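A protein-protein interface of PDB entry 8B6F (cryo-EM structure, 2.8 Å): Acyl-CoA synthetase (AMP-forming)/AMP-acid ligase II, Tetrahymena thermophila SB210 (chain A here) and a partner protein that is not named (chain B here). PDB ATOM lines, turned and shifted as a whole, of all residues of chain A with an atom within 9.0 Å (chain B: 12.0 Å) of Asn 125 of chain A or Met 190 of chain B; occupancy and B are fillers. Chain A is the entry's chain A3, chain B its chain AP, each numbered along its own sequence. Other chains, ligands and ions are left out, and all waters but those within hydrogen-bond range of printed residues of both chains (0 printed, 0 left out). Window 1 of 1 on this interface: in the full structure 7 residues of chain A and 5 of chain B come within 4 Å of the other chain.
The backbone NH (N) of Ser 126 of chain A sits close to the guanidinium group (NH2) of Arg 193 of chain B (3.4 Å).
The backbone carbonyl oxygen (O) of Met 190 of chain B sits at hydrogen-bond distance from the side-chain amide nitrogen (ND2) of Asn 125 of chain A.
The side-chain carboxylate (OD1) of Asp 188 of chain B lies within hydrogen-bond range of the side-chain hydroxyl (OH) of Tyr 169 of chain A, at 2.6 Å.
The backbone carbonyl oxygen of Ser 191 of chain B sits close to the side-chain amide oxygen of Asn 125 of chain A (2.6 Å).
NZ of Lys 132 of chain A lies within hydrogen-bond range of O of Ser 191 of chain B (3.4 Å).
Printed residues of chain A that touch a printed residue of chain B: Asn 78, His 79, Asn 125, Ser 126, Lys 132, Phe 168 and Tyr 169.
Hydrophobic or aromatic side chains of chain A that line the printed part of chain B: His 79, Phe 168 and Tyr 169.
Printed residues of chain B that touch a printed residue of chain A: Asp 188, Met 190, Ser 191, Ile 192 and Arg 193.
Among the printed residues, no Asp or Glu carboxylate lies within 4 Å of a Lys or Arg side-chain nitrogen of the other chain.
Asn 125 of chain A touches just these residues of chain B: Met 190, Ser 191, Ile 192 and Arg 193.
Met 190 of chain B touches just these residues of chain A: Asn 125, Phe 168 and Tyr 169.
No residue of chain B comes within 4 Å of Ser 123 of chain A.
Pro 124 of chain A touches none of the printed residues of chain B.
Of the printed residues of chain B, Ser 126 of chain A touches Arg 193.
No residue of chain B comes within 4 Å of Lys 127 of chain A.
No residue of chain B comes within 4 Å of Gly 167 of chain A.
No residue of chain A comes within 4 Å of Asp 189 of chain B.
Ser 191 of chain B touches three residues of chain A.
Of the printed residues of chain B, Tyr 169 of chain A touches Asp 188 (2.6 Å), Met 190 (3.7 Å) and Ser 191 (3.5 Å).
Of the printed residues of chain A, Arg 193 of chain B touches Asn 78 (3.8 Å), His 79 (3.9 Å), Asn 125 (3.1 Å) and Ser 126 (3.4 Å).
Of the printed residues of chain B, Asn 78 of chain A touches Arg 193.
Printed residues of chain A within 4 Å of Ile 192 of chain B: Asn 125.
Printed residues of chain A within 4 Å of Asp 188 of chain B: Tyr 169.
The nearest residue of chain A that does not touch Met 190 of chain B is Gly 167 of chain A (6.3 Å).
OG of Ser 123 of chain A sits at hydrogen-bond distance from OG of Ser 126 of chain A, 2.6 Å away.
O of Ser 126 of chain A lies within hydrogen-bond range of N of Tyr 133 of chain A, 2.9 Å away.
NE2 of His 79 of chain A is in hydrogen-bond range of O of Thr 166 of chain A (3.3 Å).
The side-chain hydroxyl (OG) of Ser 191 of chain B sits at hydrogen-bond distance from the backbone carbonyl oxygen (O) of Asp 188 of chain B (2.8 Å).
The backbone carbonyl oxygen (O) of Tyr 169 of chain A sits at hydrogen-bond distance from a ring nitrogen (NE2) of His 165 of chain A, 2.5 Å away.
Among the printed residues, merely in contact across the chains: Asn 78 of chain A with Arg 193 of chain B, His 79 of chain A with Arg 193 of chain B, Asn 125 of chain A with Ile 192 of chain B, Asn 125 of chain A with Arg 193 of chain B, Phe 168 of chain A with Met 190 of chain B, Tyr 169 of chain A with Met 190 of chain B and Tyr 169 of chain A with Ser 191 of chain B.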
ATOM      1  N   TRP A  74      -1.783   1.956 -13.233  1.00  0.00           N
ATOM      2  CA  TRP A  74      -1.872   0.761 -14.065  1.00  0.00           C
ATOM      3  C   TRP A  74      -3.331   0.374 -14.257  1.00  0.00           C
ATOM      4  O   TRP A  74      -3.731  -0.777 -14.071  1.00  0.00           O
ATOM      5  CB  TRP A  74      -1.077  -0.384 -13.439  1.00  0.00           C
ATOM      6  CG  TRP A  74      -0.572  -1.409 -14.416  1.00  0.00           C
ATOM      7  CD1 TRP A  74      -0.250  -1.212 -15.729  1.00  0.00           C
ATOM      8  CD2 TRP A  74      -0.333  -2.796 -14.150  1.00  0.00           C
ATOM      9  NE1 TRP A  74       0.172  -2.391 -16.293  1.00  0.00           N
ATOM     10  CE2 TRP A  74       0.131  -3.378 -15.344  1.00  0.00           C
ATOM     11  CE3 TRP A  74      -0.468  -3.602 -13.014  1.00  0.00           C
ATOM     12  CZ2 TRP A  74       0.462  -4.729 -15.437  1.00  0.00           C
ATOM     13  CZ3 TRP A  74      -0.140  -4.943 -13.108  1.00  0.00           C
ATOM     14  CH2 TRP A  74       0.319  -5.493 -14.311  1.00  0.00           C
ATOM     15  N   VAL A  75      -4.150   1.351 -14.641  1.00  0.00           N
ATOM     16  CA  VAL A  75      -5.589   1.176 -14.795  1.00  0.00           C
ATOM     17  C   VAL A  75      -5.946   1.360 -16.263  1.00  0.00           C
ATOM     18  O   VAL A  75      -5.492   2.316 -16.903  1.00  0.00           O
ATOM     19  CB  VAL A  75      -6.377   2.159 -13.911  1.00  0.00           C
ATOM     20  CG1 VAL A  75      -6.320   1.724 -12.458  1.00  0.00           C
ATOM     21  CG2 VAL A  75      -5.836   3.569 -14.062  1.00  0.00           C
ATOM     22  N   GLU A  76      -6.756   0.445 -16.789  1.00  0.00           N
ATOM     23  CA  GLU A  76      -7.102   0.444 -18.202  1.00  0.00           C
ATOM     24  C   GLU A  76      -8.066   1.589 -18.515  1.00  0.00           C
ATOM     25  O   GLU A  76      -8.427   2.397 -17.655  1.00  0.00           O
ATOM     26  CB  GLU A  76      -7.708  -0.902 -18.593  1.00  0.00           C
ATOM     27  CG  GLU A  76      -7.348  -1.384 -19.995  1.00  0.00           C
ATOM     28  CD  GLU A  76      -5.859  -1.603 -20.180  1.00  0.00           C
ATOM     29  OE1 GLU A  76      -5.113  -1.513 -19.181  1.00  0.00           O
ATOM     30  OE2 GLU A  76      -5.435  -1.863 -21.325  1.00  0.00           O
ATOM     31  N   ASN A  78     -11.272   1.683 -19.324  1.00  0.00           N
ATOM     32  CA  ASN A  78     -12.652   1.677 -18.846  1.00  0.00           C
ATOM     33  C   ASN A  78     -12.814   2.441 -17.539  1.00  0.00           C
ATOM     34  O   ASN A  78     -13.901   2.958 -17.257  1.00  0.00           O
ATOM     35  CB  ASN A  78     -13.139   0.238 -18.669  1.00  0.00           C
ATOM     36  CG  ASN A  78     -13.430  -0.442 -19.988  1.00  0.00           C
ATOM     37  OD1 ASN A  78     -13.815   0.204 -20.962  1.00  0.00           O
ATOM     38  ND2 ASN A  78     -13.255  -1.758 -20.026  1.00  0.00           N
ATOM     39  N   HIS A  79     -11.763   2.524 -16.729  1.00  0.00           N
ATOM     40  CA  HIS A  79     -11.843   3.177 -15.422  1.00  0.00           C
ATOM     41  C   HIS A  79     -11.515   4.667 -15.543  1.00  0.00           C
ATOM     42  O   HIS A  79     -10.624   5.201 -14.886  1.00  0.00           O
ATOM     43  CB  HIS A  79     -10.921   2.479 -14.432  1.00  0.00           C
ATOM     44  CG  HIS A  79     -11.266   1.042 -14.201  1.00  0.00           C
ATOM     45  ND1 HIS A  79     -11.225   0.096 -15.204  1.00  0.00           N
ATOM     46  CD2 HIS A  79     -11.667   0.389 -13.085  1.00  0.00           C
ATOM     47  CE1 HIS A  79     -11.582  -1.078 -14.713  1.00  0.00           C
ATOM     48  NE2 HIS A  79     -11.857  -0.928 -13.430  1.00  0.00           N
ATOM     49  N   LEU A 122      -3.998   0.097  -9.569  1.00  0.00           N
ATOM     50  CA  LEU A 122      -4.091  -0.718 -10.767  1.00  0.00           C
ATOM     51  C   LEU A 122      -5.520  -1.210 -10.942  1.00  0.00           C
ATOM     52  O   LEU A 122      -6.355  -1.107 -10.041  1.00  0.00           O
ATOM     53  CB  LEU A 122      -3.121  -1.899 -10.700  1.00  0.00           C
ATOM     54  CG  LEU A 122      -3.371  -2.884  -9.559  1.00  0.00           C
ATOM     55  CD1 LEU A 122      -4.201  -4.078 -10.016  1.00  0.00           C
ATOM     56  CD2 LEU A 122      -2.055  -3.314  -8.966  1.00  0.00           C
ATOM     57  N   SER A 123      -5.788  -1.746 -12.126  1.00  0.00           N
ATOM     58  CA  SER A 123      -7.067  -2.365 -12.449  1.00  0.00           C
ATOM     59  C   SER A 123      -6.895  -3.879 -12.465  1.00  0.00           C
ATOM     60  O   SER A 123      -6.205  -4.407 -13.351  1.00  0.00           O
ATOM     61  CB  SER A 123      -7.581  -1.857 -13.794  1.00  0.00           C
ATOM     62  OG  SER A 123      -6.645  -2.106 -14.820  1.00  0.00           O
ATOM     63  N   PRO A 124      -7.500  -4.621 -11.533  1.00  0.00           N
ATOM     64  CA  PRO A 124      -7.163  -6.051 -11.419  1.00  0.00           C
ATOM     65  C   PRO A 124      -7.648  -6.896 -12.582  1.00  0.00           C
ATOM     66  O   PRO A 124      -6.900  -7.752 -13.068  1.00  0.00           O
ATOM     67  CB  PRO A 124      -7.835  -6.455 -10.100  1.00  0.00           C
ATOM     68  CG  PRO A 124      -8.989  -5.533  -9.976  1.00  0.00           C
ATOM     69  CD  PRO A 124      -8.552  -4.226 -10.579  1.00  0.00           C
ATOM     70  N   ASN A 125      -8.879  -6.687 -13.046  1.00  0.00           N
ATOM     71  CA  ASN A 125      -9.445  -7.555 -14.071  1.00  0.00           C
ATOM     72  C   ASN A 125      -8.806  -7.367 -15.441  1.00  0.00           C
ATOM     73  O   ASN A 125      -9.019  -8.208 -16.319  1.00  0.00           O
ATOM     74  CB  ASN A 125     -10.951  -7.313 -14.169  1.00  0.00           C
ATOM     75  CG  ASN A 125     -11.678  -7.665 -12.888  1.00  0.00           C
ATOM     76  OD1 ASN A 125     -11.338  -8.639 -12.218  1.00  0.00           O
ATOM     77  ND2 ASN A 125     -12.678  -6.865 -12.534  1.00  0.00           N
ATOM     78  N   SER A 126      -8.036  -6.302 -15.647  1.00  0.00           N
ATOM     79  CA  SER A 126      -7.394  -6.093 -16.938  1.00  0.00           C
ATOM     80  C   SER A 126      -6.440  -7.237 -17.248  1.00  0.00           C
ATOM     81  O   SER A 126      -5.740  -7.743 -16.366  1.00  0.00           O
ATOM     82  CB  SER A 126      -6.640  -4.769 -16.960  1.00  0.00           C
ATOM     83  OG  SER A 126      -7.504  -3.699 -16.640  1.00  0.00           O
ATOM     84  N   LYS A 127      -6.413  -7.641 -18.512  1.00  0.00           N
ATOM     85  CA  LYS A 127      -5.643  -8.795 -18.953  1.00  0.00           C
ATOM     86  C   LYS A 127      -4.383  -8.320 -19.668  1.00  0.00           C
ATOM     87  O   LYS A 127      -4.464  -7.564 -20.643  1.00  0.00           O
ATOM     88  CB  LYS A 127      -6.482  -9.674 -19.879  1.00  0.00           C
ATOM     89  CG  LYS A 127      -5.806 -10.977 -20.271  1.00  0.00           C
ATOM     90  CD  LYS A 127      -6.652 -11.777 -21.256  1.00  0.00           C
ATOM     91  CE  LYS A 127      -7.991 -12.193 -20.658  1.00  0.00           C
ATOM     92  NZ  LYS A 127      -7.838 -12.938 -19.379  1.00  0.00           N
ATOM     93  N   ALA A 128      -3.227  -8.766 -19.182  1.00  0.00           N
ATOM     94  CA  ALA A 128      -1.934  -8.497 -19.804  1.00  0.00           C
ATOM     95  C   ALA A 128      -1.359  -9.826 -20.270  1.00  0.00           C
ATOM     96  O   ALA A 128      -1.036 -10.690 -19.448  1.00  0.00           O
ATOM     97  CB  ALA A 128      -0.984  -7.802 -18.831  1.00  0.00           C
ATOM     98  N   SER A 131      -2.083 -13.290 -18.443  1.00  0.00           N
ATOM     99  CA  SER A 131      -2.328 -13.143 -17.017  1.00  0.00           C
ATOM    100  C   SER A 131      -2.982 -11.794 -16.754  1.00  0.00           C
ATOM    101  O   SER A 131      -2.839 -10.847 -17.531  1.00  0.00           O
ATOM    102  CB  SER A 131      -1.032 -13.272 -16.204  1.00  0.00           C
ATOM    103  OG  SER A 131      -0.093 -12.278 -16.577  1.00  0.00           O
ATOM    104  N   LYS A 132      -3.709 -11.722 -15.645  1.00  0.00           N
ATOM    105  CA  LYS A 132      -4.372 -10.500 -15.223  1.00  0.00           C
ATOM    106  C   LYS A 132      -3.416  -9.622 -14.421  1.00  0.00           C
ATOM    107  O   LYS A 132      -2.354 -10.057 -13.971  1.00  0.00           O
ATOM    108  CB  LYS A 132      -5.614 -10.828 -14.394  1.00  0.00           C
ATOM    109  CG  LYS A 132      -6.650 -11.651 -15.141  1.00  0.00           C
ATOM    110  CD  LYS A 132      -7.872 -11.918 -14.277  1.00  0.00           C
ATOM    111  CE  LYS A 132      -8.936 -12.679 -15.054  1.00  0.00           C
ATOM    112  NZ  LYS A 132     -10.152 -12.936 -14.232  1.00  0.00           N
ATOM    113  N   TYR A 133      -3.813  -8.361 -14.238  1.00  0.00           N
ATOM    114  CA  TYR A 133      -2.977  -7.425 -13.493  1.00  0.00           C
ATOM    115  C   TYR A 133      -2.764  -7.897 -12.061  1.00  0.00           C
ATOM    116  O   TYR A 133      -1.641  -7.855 -11.548  1.00  0.00           O
ATOM    117  CB  TYR A 133      -3.604  -6.031 -13.496  1.00  0.00           C
ATOM    118  CG  TYR A 133      -3.475  -5.269 -14.799  1.00  0.00           C
ATOM    119  CD1 TYR A 133      -3.116  -5.907 -15.980  1.00  0.00           C
ATOM    120  CD2 TYR A 133      -3.697  -3.898 -14.838  1.00  0.00           C
ATOM    121  CE1 TYR A 133      -2.993  -5.201 -17.163  1.00  0.00           C
ATOM    122  CE2 TYR A 133      -3.578  -3.185 -16.015  1.00  0.00           C
ATOM    123  CZ  TYR A 133      -3.226  -3.842 -17.173  1.00  0.00           C
ATOM    124  OH  TYR A 133      -3.103  -3.135 -18.347  1.00  0.00           O
ATOM    125  N   ILE A 134      -3.822  -8.379 -11.410  1.00  0.00           N
ATOM    126  CA  ILE A 134      -3.694  -8.828 -10.026  1.00  0.00           C
ATOM    127  C   ILE A 134      -2.769 -10.035  -9.944  1.00  0.00           C
ATOM    128  O   ILE A 134      -1.946 -10.144  -9.029  1.00  0.00           O
ATOM    129  CB  ILE A 134      -5.084  -9.124  -9.428  1.00  0.00           C
ATOM    130  CG1 ILE A 134      -4.980  -9.423  -7.929  1.00  0.00           C
ATOM    131  CG2 ILE A 134      -5.756 -10.288 -10.146  1.00  0.00           C
ATOM    132  CD1 ILE A 134      -4.499  -8.251  -7.094  1.00  0.00           C
ATOM    133  N   GLU A 135      -2.890 -10.963 -10.895  1.00  0.00           N
ATOM    134  CA  GLU A 135      -2.009 -12.124 -10.907  1.00  0.00           C
ATOM    135  C   GLU A 135      -0.555 -11.710 -11.108  1.00  0.00           C
ATOM    136  O   GLU A 135       0.345 -12.234 -10.442  1.00  0.00           O
ATOM    137  CB  GLU A 135      -2.444 -13.103 -11.997  1.00  0.00           C
ATOM    138  CG  GLU A 135      -3.832 -13.683 -11.780  1.00  0.00           C
ATOM    139  CD  GLU A 135      -4.197 -14.716 -12.826  1.00  0.00           C
ATOM    140  OE1 GLU A 135      -3.401 -14.915 -13.766  1.00  0.00           O
ATOM    141  OE2 GLU A 135      -5.277 -15.332 -12.706  1.00  0.00           O
ATOM    142  N   HIS A 165      -6.392  -1.622  -5.867  1.00  0.00           N
ATOM    143  CA  HIS A 165      -6.990  -2.205  -7.060  1.00  0.00           C
ATOM    144  C   HIS A 165      -8.414  -1.693  -7.220  1.00  0.00           C
ATOM    145  O   HIS A 165      -9.163  -1.601  -6.244  1.00  0.00           O
ATOM    146  CB  HIS A 165      -6.996  -3.740  -7.002  1.00  0.00           C
ATOM    147  CG  HIS A 165      -7.922  -4.311  -5.971  1.00  0.00           C
ATOM    148  ND1 HIS A 165      -8.043  -3.790  -4.699  1.00  0.00           N
ATOM    149  CD2 HIS A 165      -8.779  -5.357  -6.031  1.00  0.00           C
ATOM    150  CE1 HIS A 165      -8.932  -4.494  -4.021  1.00  0.00           C
ATOM    151  NE2 HIS A 165      -9.393  -5.450  -4.806  1.00  0.00           N
ATOM    152  N   THR A 166      -8.777  -1.356  -8.454  1.00  0.00           N
ATOM    153  CA  THR A 166     -10.125  -0.883  -8.766  1.00  0.00           C
ATOM    154  C   THR A 166     -10.972  -2.062  -9.246  1.00  0.00           C
ATOM    155  O   THR A 166     -11.331  -2.182 -10.417  1.00  0.00           O
ATOM    156  CB  THR A 166     -10.070   0.231  -9.806  1.00  0.00           C
ATOM    157  OG1 THR A 166      -9.559  -0.285 -11.041  1.00  0.00           O
ATOM    158  CG2 THR A 166      -9.176   1.362  -9.329  1.00  0.00           C
ATOM    159  N   GLY A 167     -11.291  -2.946  -8.296  1.00  0.00           N
ATOM    160  CA  GLY A 167     -12.040  -4.146  -8.601  1.00  0.00           C
ATOM    161  C   GLY A 167     -13.077  -4.434  -7.535  1.00  0.00           C
ATOM    162  O   GLY A 167     -13.048  -3.872  -6.438  1.00  0.00           O
ATOM    163  N   PHE A 168     -14.004  -5.328  -7.884  1.00  0.00           N
ATOM    164  CA  PHE A 168     -15.085  -5.673  -6.968  1.00  0.00           C
ATOM    165  C   PHE A 168     -14.584  -6.529  -5.810  1.00  0.00           C
ATOM    166  O   PHE A 168     -14.948  -6.289  -4.653  1.00  0.00           O
ATOM    167  CB  PHE A 168     -16.197  -6.394  -7.730  1.00  0.00           C
ATOM    168  CG  PHE A 168     -17.303  -6.903  -6.852  1.00  0.00           C
ATOM    169  CD1 PHE A 168     -18.229  -6.026  -6.306  1.00  0.00           C
ATOM    170  CD2 PHE A 168     -17.434  -8.257  -6.590  1.00  0.00           C
ATOM    171  CE1 PHE A 168     -19.253  -6.490  -5.502  1.00  0.00           C
ATOM    172  CE2 PHE A 168     -18.457  -8.728  -5.788  1.00  0.00           C
ATOM    173  CZ  PHE A 168     -19.368  -7.843  -5.244  1.00  0.00           C
ATOM    174  N   TYR A 169     -13.755  -7.529  -6.099  1.00  0.00           N
ATOM    175  CA  TYR A 169     -13.261  -8.430  -5.071  1.00  0.00           C
ATOM    176  C   TYR A 169     -12.090  -7.801  -4.319  1.00  0.00           C
ATOM    177  O   TYR A 169     -11.518  -6.788  -4.731  1.00  0.00           O
ATOM    178  CB  TYR A 169     -12.838  -9.761  -5.687  1.00  0.00           C
ATOM    179  CG  TYR A 169     -13.980 -10.559  -6.272  1.00  0.00           C
ATOM    180  CD1 TYR A 169     -14.719 -11.429  -5.483  1.00  0.00           C
ATOM    181  CD2 TYR A 169     -14.316 -10.445  -7.613  1.00  0.00           C
ATOM    182  CE1 TYR A 169     -15.764 -12.164  -6.013  1.00  0.00           C
ATOM    183  CE2 TYR A 169     -15.357 -11.173  -8.154  1.00  0.00           C
ATOM    184  CZ  TYR A 169     -16.078 -12.032  -7.349  1.00  0.00           C
ATOM    185  OH  TYR A 169     -17.116 -12.760  -7.880  1.00  0.00           O
ATOM    186  N   PHE A 171      -8.302  -8.678  -2.281  1.00  0.00           N
ATOM    187  CA  PHE A 171      -7.181  -9.599  -2.227  1.00  0.00           C
ATOM    188  C   PHE A 171      -6.255  -9.208  -1.085  1.00  0.00           C
ATOM    189  O   PHE A 171      -6.177  -8.031  -0.722  1.00  0.00           O
ATOM    190  CB  PHE A 171      -6.399  -9.596  -3.548  1.00  0.00           C
ATOM    191  CG  PHE A 171      -7.271  -9.696  -4.764  1.00  0.00           C
ATOM    192  CD1 PHE A 171      -7.765 -10.922  -5.181  1.00  0.00           C
ATOM    193  CD2 PHE A 171      -7.598  -8.565  -5.493  1.00  0.00           C
ATOM    194  CE1 PHE A 171      -8.569 -11.017  -6.301  1.00  0.00           C
ATOM    195  CE2 PHE A 171      -8.402  -8.652  -6.613  1.00  0.00           C
ATOM    196  CZ  PHE A 171      -8.887  -9.880  -7.018  1.00  0.00           C
ATOM    197  N   PRO B 185     -22.725 -23.027 -13.793  1.00  0.00           N
ATOM    198  CA  PRO B 185     -22.930 -22.473 -15.141  1.00  0.00           C
ATOM    199  C   PRO B 185     -22.856 -20.960 -15.185  1.00  0.00           C
ATOM    200  O   PRO B 185     -22.441 -20.398 -16.207  1.00  0.00           O
ATOM    201  CB  PRO B 185     -24.330 -22.978 -15.519  1.00  0.00           C
ATOM    202  CG  PRO B 185     -24.554 -24.170 -14.663  1.00  0.00           C
ATOM    203  CD  PRO B 185     -23.847 -23.887 -13.378  1.00  0.00           C
ATOM    204  N   PHE B 186     -23.246 -20.282 -14.110  1.00  0.00           N
ATOM    205  CA  PHE B 186     -23.283 -18.828 -14.116  1.00  0.00           C
ATOM    206  C   PHE B 186     -21.881 -18.253 -14.268  1.00  0.00           C
ATOM    207  O   PHE B 186     -20.893 -18.817 -13.791  1.00  0.00           O
ATOM    208  CB  PHE B 186     -23.926 -18.308 -12.831  1.00  0.00           C
ATOM    209  CG  PHE B 186     -25.336 -18.777 -12.633  1.00  0.00           C
ATOM    210  CD1 PHE B 186     -26.392 -18.093 -13.211  1.00  0.00           C
ATOM    211  CD2 PHE B 186     -25.605 -19.901 -11.871  1.00  0.00           C
ATOM    212  CE1 PHE B 186     -27.691 -18.522 -13.033  1.00  0.00           C
ATOM    213  CE2 PHE B 186     -26.902 -20.335 -11.689  1.00  0.00           C
ATOM    214  CZ  PHE B 186     -27.947 -19.644 -12.271  1.00  0.00           C
ATOM    215  N   ILE B 187     -21.805 -17.115 -14.940  1.00  0.00           N
ATOM    216  CA  ILE B 187     -20.540 -16.453 -15.230  1.00  0.00           C
ATOM    217  C   ILE B 187     -20.228 -15.467 -14.116  1.00  0.00           C
ATOM    218  O   ILE B 187     -21.104 -14.728 -13.652  1.00  0.00           O
ATOM    219  CB  ILE B 187     -20.600 -15.751 -16.600  1.00  0.00           C
ATOM    220  CG1 ILE B 187     -20.835 -16.780 -17.709  1.00  0.00           C
ATOM    221  CG2 ILE B 187     -19.319 -14.977 -16.859  1.00  0.00           C
ATOM    222  CD1 ILE B 187     -21.098 -16.171 -19.072  1.00  0.00           C
ATOM    223  N   ASP B 188     -18.967 -15.455 -13.682  1.00  0.00           N
ATOM    224  CA  ASP B 188     -18.497 -14.516 -12.664  1.00  0.00           C
ATOM    225  C   ASP B 188     -18.121 -13.214 -13.366  1.00  0.00           C
ATOM    226  O   ASP B 188     -16.960 -12.941 -13.678  1.00  0.00           O
ATOM    227  CB  ASP B 188     -17.326 -15.102 -11.888  1.00  0.00           C
ATOM    228  CG  ASP B 188     -16.965 -14.279 -10.668  1.00  0.00           C
ATOM    229  OD1 ASP B 188     -17.639 -13.258 -10.417  1.00  0.00           O
ATOM    230  OD2 ASP B 188     -16.006 -14.651  -9.960  1.00  0.00           O
ATOM    231  N   ASP B 189     -19.142 -12.393 -13.616  1.00  0.00           N
ATOM    232  CA  ASP B 189     -18.942 -11.170 -14.389  1.00  0.00           C
ATOM    233  C   ASP B 189     -17.991 -10.212 -13.683  1.00  0.00           C
ATOM    234  O   ASP B 189     -17.153  -9.572 -14.328  1.00  0.00           O
ATOM    235  CB  ASP B 189     -20.286 -10.493 -14.653  1.00  0.00           C
ATOM    236  CG  ASP B 189     -21.024 -10.141 -13.376  1.00  0.00           C
ATOM    237  OD1 ASP B 189     -20.838 -10.852 -12.366  1.00  0.00           O
ATOM    238  OD2 ASP B 189     -21.790  -9.156 -13.381  1.00  0.00           O
ATOM    239  N   MET B 190     -18.103 -10.100 -12.358  1.00  0.00           N
ATOM    240  CA  MET B 190     -17.240  -9.175 -11.628  1.00  0.00           C
ATOM    241  C   MET B 190     -15.775  -9.570 -11.756  1.00  0.00           C
ATOM    242  O   MET B 190     -14.908  -8.711 -11.950  1.00  0.00           O
ATOM    243  CB  MET B 190     -17.652  -9.123 -10.157  1.00  0.00           C
ATOM    244  CG  MET B 190     -19.120  -8.788  -9.937  1.00  0.00           C
ATOM    245  SD  MET B 190     -19.670  -7.334 -10.854  1.00  0.00           S
ATOM    246  CE  MET B 190     -18.564  -6.081 -10.220  1.00  0.00           C
ATOM    247  N   SER B 191     -15.474 -10.864 -11.643  1.00  0.00           N
ATOM    248  CA  SER B 191     -14.092 -11.304 -11.804  1.00  0.00           C
ATOM    249  C   SER B 191     -13.614 -11.107 -13.239  1.00  0.00           C
ATOM    250  O   SER B 191     -12.490 -10.645 -13.464  1.00  0.00           O
ATOM    251  CB  SER B 191     -13.958 -12.769 -11.390  1.00  0.00           C
ATOM    252  OG  SER B 191     -14.611 -13.622 -12.314  1.00  0.00           O
ATOM    253  N   ILE B 192     -14.452 -11.447 -14.221  1.00  0.00           N
ATOM    254  CA  ILE B 192     -14.031 -11.355 -15.618  1.00  0.00           C
ATOM    255  C   ILE B 192     -13.765  -9.905 -16.001  1.00  0.00           C
ATOM    256  O   ILE B 192     -12.775  -9.598 -16.675  1.00  0.00           O
ATOM    257  CB  ILE B 192     -15.083 -12.002 -16.538  1.00  0.00           C
ATOM    258  CG1 ILE B 192     -15.081 -13.521 -16.342  1.00  0.00           C
ATOM    259  CG2 ILE B 192     -14.822 -11.639 -18.003  1.00  0.00           C
ATOM    260  CD1 ILE B 192     -16.123 -14.251 -17.158  1.00  0.00           C
ATOM    261  N   ARG B 193     -14.643  -8.996 -15.589  1.00  0.00           N
ATOM    262  CA  ARG B 193     -14.505  -7.587 -15.939  1.00  0.00           C
ATOM    263  C   ARG B 193     -14.827  -6.700 -14.743  1.00  0.00           C
ATOM    264  O   ARG B 193     -15.959  -6.245 -14.587  1.00  0.00           O
ATOM    265  CB  ARG B 193     -15.421  -7.240 -17.115  1.00  0.00           C
ATOM    266  CG  ARG B 193     -15.363  -5.782 -17.565  1.00  0.00           C
ATOM    267  CD  ARG B 193     -14.004  -5.419 -18.150  1.00  0.00           C
ATOM    268  NE  ARG B 193     -13.005  -5.153 -17.123  1.00  0.00           N
ATOM    269  CZ  ARG B 193     -11.751  -4.797 -17.370  1.00  0.00           C
ATOM    270  NH1 ARG B 193     -11.303  -4.662 -18.608  1.00  0.00           N
ATOM    271  NH2 ARG B 193     -10.928  -4.570 -16.351  1.00  0.00           N
